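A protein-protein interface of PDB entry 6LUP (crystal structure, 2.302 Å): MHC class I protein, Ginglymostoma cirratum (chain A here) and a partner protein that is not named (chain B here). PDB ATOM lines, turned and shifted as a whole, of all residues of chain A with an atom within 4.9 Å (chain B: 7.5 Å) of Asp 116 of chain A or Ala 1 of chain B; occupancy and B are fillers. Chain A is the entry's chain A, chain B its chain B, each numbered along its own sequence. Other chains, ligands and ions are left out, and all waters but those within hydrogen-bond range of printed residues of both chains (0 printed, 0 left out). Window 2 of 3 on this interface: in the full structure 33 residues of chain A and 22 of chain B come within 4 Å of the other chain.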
ATOM      1  N   GLN A  85      -8.910  12.313 -19.381  1.00  0.00           N
ATOM      2  CA  GLN A  85      -9.383  13.144 -20.513  1.00  0.00           C
ATOM      3  C   GLN A  85      -9.988  12.157 -21.504  1.00  0.00           C
ATOM      4  O   GLN A  85      -9.479  11.032 -21.585  1.00  0.00           O
ATOM      5  CB  GLN A  85      -8.222  13.903 -21.142  1.00  0.00           C
ATOM      6  CG  GLN A  85      -7.449  14.755 -20.156  1.00  0.00           C
ATOM      7  CD  GLN A  85      -7.112  16.094 -20.756  1.00  0.00           C
ATOM      8  OE1 GLN A  85      -7.935  16.725 -21.402  1.00  0.00           O
ATOM      9  NE2 GLN A  85      -5.888  16.538 -20.538  1.00  0.00           N
ATOM     10  N   ILE A  89      -8.353  17.830 -28.523  1.00  0.00           N
ATOM     11  CA  ILE A  89      -7.110  17.953 -29.279  1.00  0.00           C
ATOM     12  C   ILE A  89      -5.920  17.811 -28.331  1.00  0.00           C
ATOM     13  O   ILE A  89      -5.812  18.552 -27.352  1.00  0.00           O
ATOM     14  CB  ILE A  89      -7.056  19.284 -30.061  1.00  0.00           C
ATOM     15  CG1 ILE A  89      -8.191  19.332 -31.090  1.00  0.00           C
ATOM     16  CG2 ILE A  89      -5.709  19.453 -30.756  1.00  0.00           C
ATOM     17  CD1 ILE A  89      -8.725  20.721 -31.370  1.00  0.00           C
ATOM     18  N   HIS A  90      -5.041  16.852 -28.619  1.00  0.00           N
ATOM     19  CA  HIS A  90      -3.921  16.543 -27.726  1.00  0.00           C
ATOM     20  C   HIS A  90      -2.572  16.359 -28.426  1.00  0.00           C
ATOM     21  O   HIS A  90      -2.511  16.079 -29.623  1.00  0.00           O
ATOM     22  CB  HIS A  90      -4.256  15.332 -26.854  1.00  0.00           C
ATOM     23  CG  HIS A  90      -5.445  15.548 -25.973  1.00  0.00           C
ATOM     24  ND1 HIS A  90      -5.425  16.406 -24.895  1.00  0.00           N
ATOM     25  CD2 HIS A  90      -6.698  15.036 -26.025  1.00  0.00           C
ATOM     26  CE1 HIS A  90      -6.611  16.406 -24.312  1.00  0.00           C
ATOM     27  NE2 HIS A  90      -7.402  15.583 -24.977  1.00  0.00           N
ATOM     28  N   THR A  91      -1.500  16.514 -27.652  1.00  0.00           N
ATOM     29  CA  THR A  91      -0.140  16.559 -28.178  1.00  0.00           C
ATOM     30  C   THR A  91       0.834  15.768 -27.308  1.00  0.00           C
ATOM     31  O   THR A  91       0.719  15.750 -26.079  1.00  0.00           O
ATOM     32  CB  THR A  91       0.351  18.022 -28.273  1.00  0.00           C
ATOM     33  OG1 THR A  91      -0.495  18.747 -29.169  1.00  0.00           O
ATOM     34  CG2 THR A  91       1.772  18.105 -28.790  1.00  0.00           C
ATOM     35  N   GLN A  93       5.214  15.536 -27.100  1.00  0.00           N
ATOM     36  CA  GLN A  93       6.449  16.134 -27.590  1.00  0.00           C
ATOM     37  C   GLN A  93       7.679  15.481 -26.983  1.00  0.00           C
ATOM     38  O   GLN A  93       7.670  15.093 -25.815  1.00  0.00           O
ATOM     39  CB  GLN A  93       6.465  17.635 -27.313  1.00  0.00           C
ATOM     40  CG  GLN A  93       5.509  18.432 -28.180  1.00  0.00           C
ATOM     41  CD  GLN A  93       5.271  19.825 -27.643  1.00  0.00           C
ATOM     42  OE1 GLN A  93       4.533  20.017 -26.676  1.00  0.00           O
ATOM     43  NE2 GLN A  93       5.894  20.810 -28.272  1.00  0.00           N
ATOM     44  N   ALA A 114       7.049  15.850 -23.179  1.00  0.00           N
ATOM     45  CA  ALA A 114       5.928  16.687 -22.768  1.00  0.00           C
ATOM     46  C   ALA A 114       4.594  16.172 -23.273  1.00  0.00           C
ATOM     47  O   ALA A 114       4.478  15.678 -24.399  1.00  0.00           O
ATOM     48  CB  ALA A 114       6.126  18.121 -23.215  1.00  0.00           C
ATOM     49  N   TRP A 115       3.596  16.305 -22.408  1.00  0.00           N
ATOM     50  CA  TRP A 115       2.215  15.978 -22.712  1.00  0.00           C
ATOM     51  C   TRP A 115       1.416  17.276 -22.702  1.00  0.00           C
ATOM     52  O   TRP A 115       1.479  18.045 -21.738  1.00  0.00           O
ATOM     53  CB  TRP A 115       1.695  14.978 -21.677  1.00  0.00           C
ATOM     54  CG  TRP A 115       0.209  14.927 -21.513  1.00  0.00           C
ATOM     55  CD1 TRP A 115      -0.500  15.317 -20.418  1.00  0.00           C
ATOM     56  CD2 TRP A 115      -0.752  14.450 -22.465  1.00  0.00           C
ATOM     57  NE1 TRP A 115      -1.842  15.115 -20.624  1.00  0.00           N
ATOM     58  CE2 TRP A 115      -2.026  14.586 -21.874  1.00  0.00           C
ATOM     59  CE3 TRP A 115      -0.662  13.921 -23.760  1.00  0.00           C
ATOM     60  CZ2 TRP A 115      -3.202  14.215 -22.527  1.00  0.00           C
ATOM     61  CZ3 TRP A 115      -1.838  13.551 -24.414  1.00  0.00           C
ATOM     62  CH2 TRP A 115      -3.088  13.703 -23.793  1.00  0.00           C
ATOM     63  N   ASP A 116       0.688  17.522 -23.789  1.00  0.00           N
ATOM     64  CA  ASP A 116      -0.050  18.776 -23.984  1.00  0.00           C
ATOM     65  C   ASP A 116       0.789  20.001 -23.616  1.00  0.00           C
ATOM     66  O   ASP A 116       0.345  20.870 -22.866  1.00  0.00           O
ATOM     67  CB  ASP A 116      -1.381  18.761 -23.214  1.00  0.00           C
ATOM     68  CG  ASP A 116      -2.470  17.972 -23.930  1.00  0.00           C
ATOM     69  OD1 ASP A 116      -2.259  17.552 -25.086  1.00  0.00           O
ATOM     70  OD2 ASP A 116      -3.548  17.777 -23.336  1.00  0.00           O
ATOM     71  N   SER A 117       2.007  20.045 -24.146  1.00  0.00           N
ATOM     72  CA  SER A 117       2.938  21.166 -23.966  1.00  0.00           C
ATOM     73  C   SER A 117       3.302  21.502 -22.511  1.00  0.00           C
ATOM     74  O   SER A 117       3.700  22.629 -22.209  1.00  0.00           O
ATOM     75  CB  SER A 117       2.452  22.413 -24.722  1.00  0.00           C
ATOM     76  OG  SER A 117       2.410  22.175 -26.119  1.00  0.00           O
ATOM     77  N   THR A 118       3.173  20.519 -21.620  1.00  0.00           N
ATOM     78  CA  THR A 118       3.641  20.652 -20.236  1.00  0.00           C
ATOM     79  C   THR A 118       4.603  19.515 -19.880  1.00  0.00           C
ATOM     80  O   THR A 118       4.452  18.391 -20.367  1.00  0.00           O
ATOM     81  CB  THR A 118       2.478  20.667 -19.216  1.00  0.00           C
ATOM     82  OG1 THR A 118       1.717  19.461 -19.332  1.00  0.00           O
ATOM     83  CG2 THR A 118       1.564  21.867 -19.436  1.00  0.00           C
ATOM     84  N   ALA B   1      -2.178  22.554 -21.598  1.00  0.00           N
ATOM     85  CA  ALA B   1      -2.260  24.046 -21.601  1.00  0.00           C
ATOM     86  C   ALA B   1      -2.271  24.603 -23.023  1.00  0.00           C
ATOM     87  O   ALA B   1      -1.570  24.098 -23.905  1.00  0.00           O
ATOM     88  CB  ALA B   1      -1.111  24.644 -20.800  1.00  0.00           C
ATOM     89  N   THR B   2      -3.080  25.637 -23.239  1.00  0.00           N
ATOM     90  CA  THR B   2      -3.189  26.261 -24.556  1.00  0.00           C
ATOM     91  C   THR B   2      -2.851  27.746 -24.495  1.00  0.00           C
ATOM     92  O   THR B   2      -3.295  28.462 -23.592  1.00  0.00           O
ATOM     93  CB  THR B   2      -4.587  26.074 -25.193  1.00  0.00           C
ATOM     94  OG1 THR B   2      -5.547  26.879 -24.501  1.00  0.00           O
ATOM     95  CG2 THR B   2      -5.028  24.612 -25.161  1.00  0.00           C
ATOM     96  N   SER B   3      -2.051  28.190 -25.459  1.00  0.00           N
ATOM     97  CA  SER B   3      -1.700  29.594 -25.611  1.00  0.00           C
ATOM     98  C   SER B   3      -1.976  30.027 -27.045  1.00  0.00           C
ATOM     99  O   SER B   3      -1.720  29.284 -27.988  1.00  0.00           O
ATOM    100  CB  SER B   3      -0.230  29.825 -25.257  1.00  0.00           C
ATOM    101  OG  SER B   3       0.165  31.156 -25.543  1.00  0.00           O
ATOM    102  N   PHE B  30       2.575  29.481 -29.258  1.00  0.00           N
ATOM    103  CA  PHE B  30       1.229  28.911 -29.321  1.00  0.00           C
ATOM    104  C   PHE B  30       1.191  27.411 -29.058  1.00  0.00           C
ATOM    105  O   PHE B  30       2.162  26.687 -29.318  1.00  0.00           O
ATOM    106  CB  PHE B  30       0.540  29.242 -30.654  1.00  0.00           C
ATOM    107  CG  PHE B  30       1.186  28.605 -31.856  1.00  0.00           C
ATOM    108  CD1 PHE B  30       2.278  29.203 -32.485  1.00  0.00           C
ATOM    109  CD2 PHE B  30       0.688  27.415 -32.378  1.00  0.00           C
ATOM    110  CE1 PHE B  30       2.869  28.621 -33.598  1.00  0.00           C
ATOM    111  CE2 PHE B  30       1.274  26.827 -33.488  1.00  0.00           C
ATOM    112  CZ  PHE B  30       2.365  27.432 -34.100  1.00  0.00           C
ATOM    113  N   SER B  31       0.055  26.970 -28.530  1.00  0.00           N
ATOM    114  CA  SER B  31      -0.254  25.564 -28.322  1.00  0.00           C
ATOM    115  C   SER B  31      -1.774  25.439 -28.223  1.00  0.00           C
ATOM    116  O   SER B  31      -2.431  26.338 -27.688  1.00  0.00           O
ATOM    117  CB  SER B  31       0.415  25.039 -27.050  1.00  0.00           C
ATOM    118  OG  SER B  31       0.080  25.838 -25.929  1.00  0.00           O
ATOM    119  N   PRO B  32      -2.351  24.348 -28.762  1.00  0.00           N
ATOM    120  CA  PRO B  32      -1.745  23.228 -29.487  1.00  0.00           C
ATOM    121  C   PRO B  32      -1.333  23.627 -30.914  1.00  0.00           C
ATOM    122  O   PRO B  32      -1.573  24.763 -31.317  1.00  0.00           O
ATOM    123  CB  PRO B  32      -2.870  22.176 -29.511  1.00  0.00           C
ATOM    124  CG  PRO B  32      -3.935  22.682 -28.588  1.00  0.00           C
ATOM    125  CD  PRO B  32      -3.806  24.170 -28.636  1.00  0.00           C
ATOM    126  N   TRP B  60       8.110  24.357 -24.786  1.00  0.00           N
ATOM    127  CA  TRP B  60       7.173  23.516 -25.541  1.00  0.00           C
ATOM    128  C   TRP B  60       6.263  24.272 -26.511  1.00  0.00           C
ATOM    129  O   TRP B  60       5.545  23.648 -27.297  1.00  0.00           O
ATOM    130  CB  TRP B  60       6.336  22.633 -24.608  1.00  0.00           C
ATOM    131  CG  TRP B  60       7.153  21.855 -23.636  1.00  0.00           C
ATOM    132  CD1 TRP B  60       7.264  22.080 -22.296  1.00  0.00           C
ATOM    133  CD2 TRP B  60       7.992  20.733 -23.927  1.00  0.00           C
ATOM    134  NE1 TRP B  60       8.111  21.161 -21.730  1.00  0.00           N
ATOM    135  CE2 TRP B  60       8.577  20.323 -22.710  1.00  0.00           C
ATOM    136  CE3 TRP B  60       8.305  20.030 -25.099  1.00  0.00           C
ATOM    137  CZ2 TRP B  60       9.456  19.239 -22.627  1.00  0.00           C
ATOM    138  CZ3 TRP B  60       9.178  18.951 -25.016  1.00  0.00           C
ATOM    139  CH2 TRP B  60       9.742  18.567 -23.787  1.00  0.00           C
ATOM    140  N   PHE B  62       4.985  26.240 -29.731  1.00  0.00           N
ATOM    141  CA  PHE B  62       5.280  25.955 -31.130  1.00  0.00           C
ATOM    142  C   PHE B  62       5.647  27.206 -31.920  1.00  0.00           C
ATOM    143  O   PHE B  62       5.405  28.335 -31.477  1.00  0.00           O
ATOM    144  CB  PHE B  62       4.103  25.232 -31.785  1.00  0.00           C
ATOM    145  CG  PHE B  62       3.830  23.875 -31.202  1.00  0.00           C
ATOM    146  CD1 PHE B  62       4.462  22.745 -31.711  1.00  0.00           C
ATOM    147  CD2 PHE B  62       2.941  23.721 -30.140  1.00  0.00           C
ATOM    148  CE1 PHE B  62       4.216  21.490 -31.173  1.00  0.00           C
ATOM    149  CE2 PHE B  62       2.692  22.472 -29.597  1.00  0.00           C
ATOM    150  CZ  PHE B  62       3.328  21.351 -30.118  1.00  0.00           C
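NE2 of Gln 93 of chain A sits at hydrogen-bond distance from O of Trp 60 of chain B (3.0 Å). The backbone carbonyl oxygen (O) of Asp 116 of chain A sits at hydrogen-bond distance from the backbone NH (N) of Ala 1 of chain B (3.3 Å).
N of Ser 3 of chain B sits at hydrogen-bond distance from O of Ser 31 of chain B (2.9 Å). OD2 of Asp 116 of chain A is in hydrogen-bond range of ND1 of His 90 of chain A. The backbone carbonyl oxygen of Phe 30 of chain B lies within hydrogen-bond range of the backbone NH of Phe 62 of chain B, at 2.9 Å. The side-chain amide oxygen (OE1) of Gln 93 of chain A is in hydrogen-bond range of the side-chain hydroxyl (OG) of Ser 117 of chain A (3.1 Å). OD1 of Asp 116 of chain A sits at hydrogen-bond distance from N of Thr 91 of chain A, 2.9 Å away. The side-chain hydroxyl (OG) of Ser 31 of chain B sits at hydrogen-bond distance from the backbone carbonyl oxygen (O) of Ala 1 of chain B, at 3.1 Å.
Among the printed residues, pairs that only touch across the chains: Gln 93 of chain A with Phe 62 of chain B, Ala 114 of chain A with Trp 60 of chain B, Ser 117 of chain A with Phe 62 of chain B, Ser 117 of chain A with Trp 60 of chain B, Ser 117 of chain A with Ser 31 of chain B and Thr 91 of chain A with Phe 62 of chain B.
Of the printed residues of chain B, Thr 91 of chain A touches Phe 62. Printed residues of chain B within 4 Å of Ala 114 of chain A: Trp 60 (3.3 Å). Of chain B, only Ala 1 (3.3 Å) comes within 4 Å of Asp 116 of chain A. Ala 1 of chain B touches just one residue of chain A: Asp 116 (3.3 Å). Printed residues of chain A within 4 Å of Trp 60 of chain B: Gln 93 (3.0 Å), Ala 114 (3.3 Å) and Ser 117 (3.6 Å). The nearest printed residue of chain A that does not touch Trp 60 of chain B is Thr 118 of chain A (4.3 Å).
Hydrophobic or aromatic side chains of chain A that line the printed part of chain B: Ala 114. Of the 8 printed residues of chain B, 4 touch a printed residue of chain A. Among the printed residues, 8 pairs touch across the chains. Among the printed residues, no Asp or Glu carboxylate lies within 4 Å of a Lys or Arg side-chain nitrogen of the other chain.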
